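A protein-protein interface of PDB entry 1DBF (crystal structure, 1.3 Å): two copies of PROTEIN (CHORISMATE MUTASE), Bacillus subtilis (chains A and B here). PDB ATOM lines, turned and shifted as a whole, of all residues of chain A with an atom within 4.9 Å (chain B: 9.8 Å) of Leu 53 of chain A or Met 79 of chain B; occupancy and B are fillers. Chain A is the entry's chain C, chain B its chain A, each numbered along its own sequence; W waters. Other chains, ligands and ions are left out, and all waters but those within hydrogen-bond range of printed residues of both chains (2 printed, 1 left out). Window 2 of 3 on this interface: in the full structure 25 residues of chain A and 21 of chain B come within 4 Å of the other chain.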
ATOM      1  N   VAL A  12      26.102 -20.206  22.275  1.00  0.00           N
ATOM      2  CA  VAL A  12      26.139 -21.653  22.328  1.00  0.00           C
ATOM      3  C   VAL A  12      26.887 -22.191  21.100  1.00  0.00           C
ATOM      4  O   VAL A  12      26.935 -21.521  20.049  1.00  0.00           O
ATOM      5  CB  VAL A  12      24.740 -22.302  22.373  1.00  0.00           C
ATOM      6  CG1 VAL A  12      24.082 -21.975  23.698  1.00  0.00           C
ATOM      7  CG2 VAL A  12      23.858 -21.882  21.208  1.00  0.00           C
ATOM      8  N   ASP A  15      22.716 -25.202  18.318  1.00  0.00           N
ATOM      9  CA  ASP A  15      21.316 -24.896  18.620  1.00  0.00           C
ATOM     10  C   ASP A  15      20.608 -26.109  19.223  1.00  0.00           C
ATOM     11  O   ASP A  15      19.754 -26.725  18.572  1.00  0.00           O
ATOM     12  CB  ASP A  15      20.655 -24.440  17.327  1.00  0.00           C
ATOM     13  CG  ASP A  15      19.186 -24.124  17.466  1.00  0.00           C
ATOM     14  OD1 ASP A  15      18.832 -23.713  18.584  1.00  0.00           O
ATOM     15  OD2 ASP A  15      18.417 -24.257  16.470  1.00  0.00           O
ATOM     16  N   ILE A  20      21.523 -24.403  25.064  1.00  0.00           N
ATOM     17  CA  ILE A  20      20.886 -23.103  25.319  1.00  0.00           C
ATOM     18  C   ILE A  20      20.522 -22.991  26.785  1.00  0.00           C
ATOM     19  O   ILE A  20      20.793 -21.911  27.335  1.00  0.00           O
ATOM     20  CB  ILE A  20      19.675 -22.869  24.386  1.00  0.00           C
ATOM     21  CG1 ILE A  20      20.121 -22.743  22.922  1.00  0.00           C
ATOM     22  CG2 ILE A  20      18.835 -21.681  24.821  1.00  0.00           C
ATOM     23  CD1 ILE A  20      19.030 -22.814  21.874  1.00  0.00           C
ATOM     24  N   ALA A  49      17.206 -13.910  21.175  1.00  0.00           N
ATOM     25  CA  ALA A  49      17.999 -14.934  20.484  1.00  0.00           C
ATOM     26  C   ALA A  49      18.193 -14.527  19.033  1.00  0.00           C
ATOM     27  O   ALA A  49      17.236 -13.994  18.431  1.00  0.00           O
ATOM     28  CB  ALA A  49      17.315 -16.315  20.532  1.00  0.00           C
ATOM     29  N   THR A  50      19.387 -14.761  18.535  1.00  0.00           N
ATOM     30  CA  THR A  50      19.622 -14.613  17.092  1.00  0.00           C
ATOM     31  C   THR A  50      18.745 -15.568  16.313  1.00  0.00           C
ATOM     32  O   THR A  50      18.297 -16.581  16.846  1.00  0.00           O
ATOM     33  CB  THR A  50      21.112 -14.831  16.782  1.00  0.00           C
ATOM     34  OG1 THR A  50      21.626 -15.935  17.522  1.00  0.00           O
ATOM     35  CG2 THR A  50      21.832 -13.544  17.245  1.00  0.00           C
ATOM     36  N   PRO A  51      18.453 -15.257  15.034  1.00  0.00           N
ATOM     37  CA  PRO A  51      17.475 -16.052  14.297  1.00  0.00           C
ATOM     38  C   PRO A  51      18.007 -17.425  13.913  1.00  0.00           C
ATOM     39  O   PRO A  51      17.276 -18.133  13.208  1.00  0.00           O
ATOM     40  CB  PRO A  51      17.142 -15.171  13.083  1.00  0.00           C
ATOM     41  CG  PRO A  51      18.383 -14.331  12.919  1.00  0.00           C
ATOM     42  CD  PRO A  51      18.923 -14.072  14.322  1.00  0.00           C
ATOM     43  N   ASP A  52      19.199 -17.807  14.373  1.00  0.00           N
ATOM     44  CA  ASP A  52      19.739 -19.144  14.108  1.00  0.00           C
ATOM     45  C   ASP A  52      19.415 -20.083  15.279  1.00  0.00           C
ATOM     46  O   ASP A  52      19.822 -21.253  15.185  1.00  0.00           O
ATOM     47  CB  ASP A  52      21.240 -19.156  13.835  1.00  0.00           C
ATOM     48  CG  ASP A  52      22.022 -18.312  14.831  1.00  0.00           C
ATOM     49  OD1 ASP A  52      21.440 -17.962  15.889  1.00  0.00           O
ATOM     50  OD2 ASP A  52      23.201 -18.007  14.555  1.00  0.00           O
ATOM     51  N   LEU A  53      18.702 -19.574  16.286  1.00  0.00           N
ATOM     52  CA  LEU A  53      18.377 -20.422  17.460  1.00  0.00           C
ATOM     53  C   LEU A  53      16.906 -20.758  17.516  1.00  0.00           C
ATOM     54  O   LEU A  53      16.054 -19.857  17.556  1.00  0.00           O
ATOM     55  CB  LEU A  53      18.860 -19.699  18.733  1.00  0.00           C
ATOM     56  CG  LEU A  53      20.375 -19.521  18.859  1.00  0.00           C
ATOM     57  CD1 LEU A  53      20.692 -18.824  20.187  1.00  0.00           C
ATOM     58  CD2 LEU A  53      21.144 -20.838  18.727  1.00  0.00           C
ATOM     59  N   HIS A  54      16.566 -22.034  17.500  1.00  0.00           N
ATOM     60  CA  HIS A  54      15.162 -22.443  17.477  1.00  0.00           C
ATOM     61  C   HIS A  54      14.875 -23.531  18.474  1.00  0.00           C
ATOM     62  O   HIS A  54      13.699 -23.941  18.623  1.00  0.00           O
ATOM     63  CB  HIS A  54      14.789 -22.990  16.084  1.00  0.00           C
ATOM     64  CG  HIS A  54      15.204 -22.085  14.982  1.00  0.00           C
ATOM     65  ND1 HIS A  54      14.495 -20.934  14.691  1.00  0.00           N
ATOM     66  CD2 HIS A  54      16.264 -22.122  14.149  1.00  0.00           C
ATOM     67  CE1 HIS A  54      15.080 -20.295  13.687  1.00  0.00           C
ATOM     68  NE2 HIS A  54      16.150 -21.006  13.344  1.00  0.00           N
ATOM     69  N   ALA A  55      15.866 -24.081  19.172  1.00  0.00           N
ATOM     70  CA  ALA A  55      15.563 -25.331  19.896  1.00  0.00           C
ATOM     71  C   ALA A  55      14.684 -25.133  21.137  1.00  0.00           C
ATOM     72  O   ALA A  55      13.987 -26.075  21.522  1.00  0.00           O
ATOM     73  CB  ALA A  55      16.870 -26.036  20.220  1.00  0.00           C
ATOM     74  N   VAL A  56      14.697 -23.981  21.781  1.00  0.00           N
ATOM     75  CA  VAL A  56      13.984 -23.742  23.025  1.00  0.00           C
ATOM     76  C   VAL A  56      13.894 -22.240  23.249  1.00  0.00           C
ATOM     77  O   VAL A  56      14.761 -21.524  22.694  1.00  0.00           O
ATOM     78  CB  VAL A  56      14.699 -24.459  24.219  1.00  0.00           C
ATOM     79  CG1 VAL A  56      16.005 -23.743  24.582  1.00  0.00           C
ATOM     80  CG2 VAL A  56      13.723 -24.610  25.406  1.00  0.00           C
ATOM     81  N   PHE A  57      12.901 -21.817  24.030  1.00  0.00           N
ATOM     82  CA  PHE A  57      12.924 -20.420  24.504  1.00  0.00           C
ATOM     83  C   PHE A  57      13.964 -20.283  25.587  1.00  0.00           C
ATOM     84  O   PHE A  57      13.858 -21.029  26.583  1.00  0.00           O
ATOM     85  CB  PHE A  57      11.554 -20.027  25.076  1.00  0.00           C
ATOM     86  CG  PHE A  57      10.545 -19.929  23.919  1.00  0.00           C
ATOM     87  CD1 PHE A  57      10.507 -18.779  23.130  1.00  0.00           C
ATOM     88  CD2 PHE A  57       9.704 -21.009  23.701  1.00  0.00           C
ATOM     89  CE1 PHE A  57       9.588 -18.762  22.083  1.00  0.00           C
ATOM     90  CE2 PHE A  57       8.785 -20.982  22.649  1.00  0.00           C
ATOM     91  CZ  PHE A  57       8.753 -19.835  21.866  1.00  0.00           C
ATOM     92  N   PRO A  58      14.990 -19.400  25.507  1.00  0.00           N
ATOM     93  CA  PRO A  58      15.984 -19.346  26.578  1.00  0.00           C
ATOM     94  C   PRO A  58      15.352 -18.958  27.919  1.00  0.00           C
ATOM     95  O   PRO A  58      15.898 -19.229  29.015  1.00  0.00           O
ATOM     96  CB  PRO A  58      16.973 -18.269  26.136  1.00  0.00           C
ATOM     97  CG  PRO A  58      16.724 -18.073  24.691  1.00  0.00           C
ATOM     98  CD  PRO A  58      15.316 -18.531  24.423  1.00  0.00           C
ATOM     99  N   CYS A  75      10.569 -13.599  25.514  1.00  0.00           N
ATOM    100  CA  CYS A  75      11.673 -13.620  24.568  1.00  0.00           C
ATOM    101  C   CYS A  75      11.340 -12.820  23.301  1.00  0.00           C
ATOM    102  O   CYS A  75      10.209 -12.398  23.048  1.00  0.00           O
ATOM    103  CB  CYS A  75      12.057 -15.072  24.136  1.00  0.00           C
ATOM    104  SG  CYS A  75      12.525 -16.052  25.608  1.00  0.00           S
ATOM    105  N   MET A  76      12.402 -12.554  22.545  1.00  0.00           N
ATOM    106  CA  MET A  76      12.182 -11.951  21.224  1.00  0.00           C
ATOM    107  C   MET A  76      13.358 -12.320  20.350  1.00  0.00           C
ATOM    108  O   MET A  76      14.408 -12.754  20.831  1.00  0.00           O
ATOM    109  CB  MET A  76      11.951 -10.444  21.256  1.00  0.00           C
ATOM    110  CG  MET A  76      13.198  -9.601  21.519  1.00  0.00           C
ATOM    111  SD  MET A  76      13.614  -9.801  23.265  1.00  0.00           S
ATOM    112  CE  MET A  76      14.211  -8.134  23.558  1.00  0.00           C
ATOM    113  N   GLN A  77      13.161 -12.141  19.041  1.00  0.00           N
ATOM    114  CA  GLN A  77      14.274 -12.320  18.111  1.00  0.00           C
ATOM    115  C   GLN A  77      15.139 -11.085  18.033  1.00  0.00           C
ATOM    116  O   GLN A  77      14.621  -9.991  17.862  1.00  0.00           O
ATOM    117  CB  GLN A  77      13.727 -12.564  16.696  1.00  0.00           C
ATOM    118  CG  GLN A  77      14.794 -13.208  15.801  1.00  0.00           C
ATOM    119  CD  GLN A  77      14.083 -13.644  14.521  1.00  0.00           C
ATOM    120  OE1 GLN A  77      13.517 -14.724  14.512  1.00  0.00           O
ATOM    121  NE2 GLN A  77      14.128 -12.788  13.509  1.00  0.00           N
ATOM    122  N   LYS A  87      24.500 -17.403  17.088  1.00  0.00           N
ATOM    123  CA  LYS A  87      24.105 -18.281  18.200  1.00  0.00           C
ATOM    124  C   LYS A  87      24.191 -17.566  19.532  1.00  0.00           C
ATOM    125  O   LYS A  87      24.784 -18.108  20.474  1.00  0.00           O
ATOM    126  CB  LYS A  87      24.969 -19.556  18.217  1.00  0.00           C
ATOM    127  CG  LYS A  87      24.705 -20.445  17.021  1.00  0.00           C
ATOM    128  CD  LYS A  87      25.492 -21.773  17.114  1.00  0.00           C
ATOM    129  CE  LYS A  87      25.115 -22.527  15.845  1.00  0.00           C
ATOM    130  NZ  LYS A  87      25.915 -21.944  14.706  1.00  0.00           N
ATOM    131  N   CYS A  88      23.578 -16.394  19.585  1.00  0.00           N
ATOM    132  CA  CYS A  88      23.764 -15.553  20.756  1.00  0.00           C
ATOM    133  C   CYS A  88      22.467 -15.272  21.481  1.00  0.00           C
ATOM    134  O   CYS A  88      21.480 -14.914  20.829  1.00  0.00           O
ATOM    135  CB  CYS A  88      24.380 -14.231  20.301  1.00  0.00           C
ATOM    136  SG  CYS A  88      24.730 -13.023  21.622  1.00  0.00           S
ATOM    137  N   ILE A  89      22.570 -15.404  22.815  1.00  0.00           N
ATOM    138  CA  ILE A  89      21.457 -15.109  23.702  1.00  0.00           C
ATOM    139  C   ILE A  89      21.807 -13.836  24.474  1.00  0.00           C
ATOM    140  O   ILE A  89      22.868 -13.798  25.089  1.00  0.00           O
ATOM    141  CB  ILE A  89      21.182 -16.256  24.695  1.00  0.00           C
ATOM    142  CG1 ILE A  89      20.799 -17.586  24.047  1.00  0.00           C
ATOM    143  CG2 ILE A  89      20.110 -15.784  25.673  1.00  0.00           C
ATOM    144  CD1 ILE A  89      21.924 -18.606  24.119  1.00  0.00           C
ATOM    145  N   SER B  48       4.575  -9.159  21.603  1.00  0.00           N
ATOM    146  CA  SER B  48       5.303  -9.951  20.606  1.00  0.00           C
ATOM    147  C   SER B  48       4.297 -10.804  19.807  1.00  0.00           C
ATOM    148  O   SER B  48       3.193 -11.119  20.265  1.00  0.00           O
ATOM    149  CB  SER B  48       6.387 -10.839  21.200  1.00  0.00           C
ATOM    150  OG  SER B  48       5.790 -11.980  21.738  1.00  0.00           O
ATOM    151  N   ALA B  49       4.726 -11.102  18.560  1.00  0.00           N
ATOM    152  CA  ALA B  49       3.944 -12.014  17.730  1.00  0.00           C
ATOM    153  C   ALA B  49       4.872 -13.024  17.081  1.00  0.00           C
ATOM    154  O   ALA B  49       6.004 -12.690  16.664  1.00  0.00           O
ATOM    155  CB  ALA B  49       3.201 -11.283  16.627  1.00  0.00           C
ATOM    156  N   THR B  50       4.361 -14.265  17.012  1.00  0.00           N
ATOM    157  CA  THR B  50       5.161 -15.285  16.296  1.00  0.00           C
ATOM    158  C   THR B  50       5.239 -14.835  14.847  1.00  0.00           C
ATOM    159  O   THR B  50       4.407 -14.061  14.370  1.00  0.00           O
ATOM    160  CB  THR B  50       4.546 -16.674  16.456  1.00  0.00           C
ATOM    161  OG1 THR B  50       3.126 -16.525  16.339  1.00  0.00           O
ATOM    162  CG2 THR B  50       4.861 -17.189  17.859  1.00  0.00           C
ATOM    163  N   PRO B  51       6.237 -15.302  14.116  1.00  0.00           N
ATOM    164  CA  PRO B  51       6.391 -14.838  12.746  1.00  0.00           C
ATOM    165  C   PRO B  51       5.381 -15.363  11.749  1.00  0.00           C
ATOM    166  O   PRO B  51       5.574 -15.002  10.571  1.00  0.00           O
ATOM    167  CB  PRO B  51       7.796 -15.370  12.374  1.00  0.00           C
ATOM    168  CG  PRO B  51       7.999 -16.554  13.258  1.00  0.00           C
ATOM    169  CD  PRO B  51       7.271 -16.266  14.534  1.00  0.00           C
ATOM    170  N   ASP B  52       4.385 -16.135  12.152  1.00  0.00           N
ATOM    171  CA  ASP B  52       3.281 -16.508  11.247  1.00  0.00           C
ATOM    172  C   ASP B  52       2.188 -15.460  11.319  1.00  0.00           C
ATOM    173  O   ASP B  52       1.141 -15.608  10.692  1.00  0.00           O
ATOM    174  CB  ASP B  52       2.739 -17.893  11.602  1.00  0.00           C
ATOM    175  CG  ASP B  52       2.480 -18.040  13.104  1.00  0.00           C
ATOM    176  OD1 ASP B  52       2.399 -16.985  13.792  1.00  0.00           O
ATOM    177  OD2 ASP B  52       2.314 -19.217  13.567  1.00  0.00           O
ATOM    178  N   MET B  76       7.342  -6.535  18.868  1.00  0.00           N
ATOM    179  CA  MET B  76       8.561  -7.239  18.472  1.00  0.00           C
ATOM    180  C   MET B  76       8.184  -8.616  17.936  1.00  0.00           C
ATOM    181  O   MET B  76       7.113  -9.147  18.268  1.00  0.00           O
ATOM    182  CB  MET B  76       9.465  -7.381  19.721  1.00  0.00           C
ATOM    183  CG  MET B  76       8.821  -8.007  20.955  1.00  0.00           C
ATOM    184  SD  MET B  76       9.719  -7.696  22.473  1.00  0.00           S
ATOM    185  CE  MET B  76       8.777  -8.877  23.494  1.00  0.00           C
ATOM    186  N   GLN B  77       9.104  -9.217  17.183  1.00  0.00           N
ATOM    187  CA  GLN B  77       8.922 -10.541  16.679  1.00  0.00           C
ATOM    188  C   GLN B  77       9.393 -11.520  17.774  1.00  0.00           C
ATOM    189  O   GLN B  77      10.514 -11.433  18.253  1.00  0.00           O
ATOM    190  CB  GLN B  77       9.714 -10.793  15.392  1.00  0.00           C
ATOM    191  CG  GLN B  77       9.145 -12.034  14.710  1.00  0.00           C
ATOM    192  CD  GLN B  77       9.565 -12.004  13.250  1.00  0.00           C
ATOM    193  OE1 GLN B  77      10.507 -12.706  12.933  1.00  0.00           O
ATOM    194  NE2 GLN B  77       8.902 -11.195  12.434  1.00  0.00           N
ATOM    195  N   GLU B  78       8.504 -12.486  18.035  1.00  0.00           N
ATOM    196  CA  GLU B  78       8.853 -13.582  18.967  1.00  0.00           C
ATOM    197  C   GLU B  78       9.821 -14.492  18.216  1.00  0.00           C
ATOM    198  O   GLU B  78       9.778 -14.569  16.963  1.00  0.00           O
ATOM    199  CB  GLU B  78       7.594 -14.282  19.492  1.00  0.00           C
ATOM    200  CG  GLU B  78       7.823 -15.618  20.201  1.00  0.00           C
ATOM    201  CD  GLU B  78       8.490 -15.520  21.577  1.00  0.00           C
ATOM    202  OE1 GLU B  78       9.698 -15.155  21.532  1.00  0.00           O
ATOM    203  OE2 GLU B  78       7.864 -15.829  22.632  1.00  0.00           O
ATOM    204  N   MET B  79      10.712 -15.182  18.926  1.00  0.00           N
ATOM    205  CA  MET B  79      11.532 -16.200  18.301  1.00  0.00           C
ATOM    206  C   MET B  79      10.706 -17.302  17.665  1.00  0.00           C
ATOM    207  O   MET B  79       9.573 -17.578  18.127  1.00  0.00           O
ATOM    208  CB  MET B  79      12.286 -16.965  19.386  1.00  0.00           C
ATOM    209  CG  MET B  79      13.414 -16.270  20.072  1.00  0.00           C
ATOM    210  SD  MET B  79      13.890 -17.294  21.484  1.00  0.00           S
ATOM    211  CE  MET B  79      14.611 -18.676  20.621  1.00  0.00           C
ATOM    212  N   ASP B  80      11.297 -17.931  16.664  1.00  0.00           N
ATOM    213  CA  ASP B  80      10.668 -19.079  16.050  1.00  0.00           C
ATOM    214  C   ASP B  80      11.239 -20.345  16.679  1.00  0.00           C
ATOM    215  O   ASP B  80      12.358 -20.763  16.323  1.00  0.00           O
ATOM    216  CB  ASP B  80      10.955 -19.079  14.548  1.00  0.00           C
ATOM    217  CG  ASP B  80      10.048 -19.983  13.754  1.00  0.00           C
ATOM    218  OD1 ASP B  80       9.224 -20.716  14.350  1.00  0.00           O
ATOM    219  OD2 ASP B  80      10.162 -19.949  12.511  1.00  0.00           O
ATOM    220  N   VAL B  81      10.525 -20.961  17.598  1.00  0.00           N
ATOM    221  CA  VAL B  81      10.996 -22.188  18.213  1.00  0.00           C
ATOM    222  C   VAL B  81      10.281 -23.405  17.665  1.00  0.00           C
ATOM    223  O   VAL B  81       9.062 -23.425  17.475  1.00  0.00           O
ATOM    224  CB  VAL B  81      10.747 -22.093  19.741  1.00  0.00           C
ATOM    225  CG1 VAL B  81      10.884 -23.463  20.410  1.00  0.00           C
ATOM    226  CG2 VAL B  81      11.708 -21.015  20.266  1.00  0.00           C
ATOM    227  N   THR B  82      11.048 -24.446  17.386  1.00  0.00           N
ATOM    228  CA  THR B  82      10.553 -25.721  16.913  1.00  0.00           C
ATOM    229  C   THR B  82       9.582 -26.284  17.937  1.00  0.00           C
ATOM    230  O   THR B  82       9.947 -26.506  19.093  1.00  0.00           O
ATOM    231  CB  THR B  82      11.755 -26.681  16.747  1.00  0.00           C
ATOM    232  OG1 THR B  82      12.703 -26.053  15.867  1.00  0.00           O
ATOM    233  CG2 THR B  82      11.323 -27.998  16.131  1.00  0.00           C
ATOM    234  N   GLY B  83       8.337 -26.480  17.529  1.00  0.00           N
ATOM    235  CA  GLY B  83       7.304 -26.886  18.440  1.00  0.00           C
ATOM    236  C   GLY B  83       6.692 -25.733  19.200  1.00  0.00           C
ATOM    237  O   GLY B  83       5.789 -25.959  20.031  1.00  0.00           O
ATOM    238  N   GLY B  84       7.138 -24.499  18.958  1.00  0.00           N
ATOM    239  CA  GLY B  84       6.631 -23.395  19.777  1.00  0.00           C
ATOM    240  C   GLY B  84       5.183 -23.181  19.373  1.00  0.00           C
ATOM    241  O   GLY B  84       4.720 -23.564  18.287  1.00  0.00           O
ATOM    242  N   LEU B  85       4.423 -22.606  20.256  1.00  0.00           N
ATOM    243  CA  LEU B  85       3.001 -22.394  20.008  1.00  0.00           C
ATOM    244  C   LEU B  85       2.816 -21.475  18.800  1.00  0.00           C
ATOM    245  O   LEU B  85       3.401 -20.385  18.769  1.00  0.00           O
ATOM    246  CB  LEU B  85       2.346 -21.800  21.261  1.00  0.00           C
ATOM    247  CG  LEU B  85       0.834 -21.608  21.201  1.00  0.00           C
ATOM    248  CD1 LEU B  85       0.131 -22.968  21.095  1.00  0.00           C
ATOM    249  CD2 LEU B  85       0.258 -20.886  22.411  1.00  0.00           C
ATOM    250  N   LYS B  86       2.007 -21.851  17.843  1.00  0.00           N
ATOM    251  CA  LYS B  86       1.775 -21.037  16.658  1.00  0.00           C
ATOM    252  C   LYS B  86       0.788 -19.912  16.887  1.00  0.00           C
ATOM    253  O   LYS B  86      -0.009 -19.990  17.812  1.00  0.00           O
ATOM    254  CB  LYS B  86       1.228 -21.977  15.549  1.00  0.00           C
ATOM    255  CG  LYS B  86       2.254 -23.049  15.223  1.00  0.00           C
ATOM    256  CD  LYS B  86       3.266 -22.560  14.200  1.00  0.00           C
ATOM    257  CE  LYS B  86       3.577 -23.758  13.294  1.00  0.00           C
ATOM    258  NZ  LYS B  86       2.434 -24.731  13.367  1.00  0.00           N
ATOM    259  N   LYS B  87       0.817 -18.892  16.028  1.00  0.00           N
ATOM    260  CA  LYS B  87      -0.210 -17.825  16.002  1.00  0.00           C
ATOM    261  C   LYS B  87      -0.448 -17.262  17.385  1.00  0.00           C
ATOM    262  O   LYS B  87      -1.593 -17.098  17.844  1.00  0.00           O
ATOM    263  CB  LYS B  87      -1.502 -18.371  15.372  1.00  0.00           C
ATOM    264  CG  LYS B  87      -1.255 -18.806  13.907  1.00  0.00           C
ATOM    265  CD  LYS B  87      -2.520 -19.249  13.202  1.00  0.00           C
ATOM    266  CE  LYS B  87      -2.255 -19.876  11.839  1.00  0.00           C
ATOM    267  NZ  LYS B  87      -1.428 -21.127  11.924  1.00  0.00           N
ATOM    268  N   CYS B  88       0.651 -16.894  18.043  1.00  0.00           N
ATOM    269  CA  CYS B  88       0.584 -16.496  19.419  1.00  0.00           C
ATOM    270  C   CYS B  88       1.053 -15.072  19.604  1.00  0.00           C
ATOM    271  O   CYS B  88       2.088 -14.635  19.102  1.00  0.00           O
ATOM    272  CB  CYS B  88       1.482 -17.418  20.231  1.00  0.00           C
ATOM    273  SG  CYS B  88       1.572 -17.172  22.007  1.00  0.00           S
ATOM    274  N   ARG B  90       2.008 -12.446  22.600  1.00  0.00           N
ATOM    275  CA  ARG B  90       2.387 -12.348  24.015  1.00  0.00           C
ATOM    276  C   ARG B  90       2.494 -10.877  24.437  1.00  0.00           C
ATOM    277  O   ARG B  90       2.814 -10.013  23.603  1.00  0.00           O
ATOM    278  CB  ARG B  90       3.754 -13.037  24.261  1.00  0.00           C
ATOM    279  CG  ARG B  90       3.645 -14.563  24.028  1.00  0.00           C
ATOM    280  CD  ARG B  90       5.051 -15.140  23.992  1.00  0.00           C
ATOM    281  NE  ARG B  90       5.215 -16.585  24.025  1.00  0.00           N
ATOM    282  CZ  ARG B  90       5.193 -17.380  22.944  1.00  0.00           C
ATOM    283  NH1 ARG B  90       4.943 -16.884  21.716  1.00  0.00           N
ATOM    284  NH2 ARG B  90       5.392 -18.676  23.065  1.00  0.00           N
HETATM  285  O   HOH W   1       7.597 -12.549  23.620  1.00  0.00           O
HETATM  286  O   HOH W   2      13.652 -17.402  15.565  1.00  0.00           O
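O of Gln 77 of chain B lies within hydrogen-bond range of N of Gln 77 of chain A (2.9 Å). ND1 of His 54 of chain A is in hydrogen-bond range of O of Asp 80 of chain B. N of Thr 82 of chain B lies within hydrogen-bond range of O of His 54 of chain A. O of Cys 75 of chain A lies close to OE1 of Glu 78 of chain B, at 3.2 Å.
Met 76 of chain A touches its own counterpart, Met 76 of chain B. Met 76 of chain A touches Gln 77 of chain B, but with the chains exchanged Gln 77 of chain A does not touch Met 76 of chain B (6.1 Å). Gln 77 of chain A touches its own counterpart, Gln 77 of chain B. Of the 20 pairs that touch across the chains among the printed residues, 2 have their exchanged pair printed and touching as well.
Met 79 of chain B touches Ala 49 of chain A (CE to CB, 3.6 Å). His 54 of chain A touches Val 81 of chain B. Met 79 of chain B touches Val 56 of chain A. Val 56 of chain A touches Val 81 of chain B. Glu 78 of chain B touches Phe 57 of chain A. Arg 90 of chain B touches Phe 57 of chain A. Met 76 of chain B touches Cys 75 of chain A (CE to O, 3.8 Å). CB of Cys 75 of chain A touches SD of Met 79 of chain B, 3.9 Å away. CA of Met 76 of chain A touches O of Gln 77 of chain B (3.4 Å). Gln 77 of chain A touches Met 79 of chain B (N to N, 3.9 Å).
Water W2 lies within hydrogen-bond range of the backbone NH (N) of Asp 80 of chain B and the side-chain amide oxygen (OE1) of Gln 77 of chain A. Water W1 lies within hydrogen-bond range of the side-chain hydroxyl (OG) of Ser 48 of chain B (2.7 Å), the backbone carbonyl oxygen (O) of Cys 75 of chain A (2.7 Å) and the side-chain carboxylate (OE2) of Glu 78 of chain B (3.4 Å).
N of Ser 48 of chain B is in hydrogen-bond range of O of Arg 90 of chain B. The backbone NH of Ala 49 of chain B sits at hydrogen-bond distance from the backbone carbonyl oxygen of Met 76 of chain B (3.1 Å). The backbone NH of Glu 78 of chain B lies within hydrogen-bond range of the backbone carbonyl oxygen of Ala 49 of chain B, 2.9 Å away. SG of Cys 88 of chain B lies within hydrogen-bond range of NH1 of Arg 90 of chain B. N of Ala 49 of chain A lies within hydrogen-bond range of O of Met 76 of chain A. NE2 of His 54 of chain A lies within hydrogen-bond range of O of Pro 51 of chain A (3.1 Å).
Of the 19 printed residues of chain A, 9 touch a printed residue of chain B. Printed residues of chain A that touch a printed residue of chain B: Ala 49, Leu 53, His 54, Val 56, Phe 57, Pro 58, Cys 75, Met 76 and Gln 77. Hydrophobic or aromatic side chains of chain A within 4 Å of the printed part of chain B: Ala 49, His 54, Phe 57, Pro 58 and Met 76. Printed residues of chain B that touch a printed residue of chain A: Met 76, Gln 77, Glu 78, Met 79, Asp 80, Val 81, Thr 82 and Arg 90. Hydrophobic or aromatic side chains of chain B that line the printed part of chain A: Met 76, Met 79 and Val 81. Among the printed residues, no Asp or Glu carboxylate lies within 4 Å of a Lys or Arg side-chain nitrogen of the other chain.
Asp 15 of chain A touches none of the printed residues of chain B. Printed residues of chain B within 4 Å of Ala 49 of chain A: Met 79 (3.6 Å). Printed residues of chain B within 4 Å of Leu 53 of chain A: Met 79. Of chain B, only Asp 80 (2.7 Å), Val 81 (3.2 Å) and Thr 82 (3.0 Å) come within 4 Å of His 54 of chain A. Of the printed residues of chain B, Phe 57 of chain A touches Glu 78, Val 81 and Arg 90. Of the printed residues of chain B, Cys 75 of chain A touches Met 76 (3.8 Å), Glu 78 (3.2 Å) and Met 79 (3.9 Å). Of the printed residues of chain A, Met 79 of chain B touches Ala 49, Leu 53, Val 56, Pro 58, Cys 75, Met 76 and Gln 77. The nearest printed residue of chain B that does not touch Leu 53 of chain A is Asp 80 of chain B (4.0002 Å). The nearest printed residue of chain A that does not touch Met 79 of chain B is Phe 57 of chain A (4.04 Å). The nearest printed residue of chain B that does not touch Phe 57 of chain A is Met 79 of chain B (4.04 Å).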
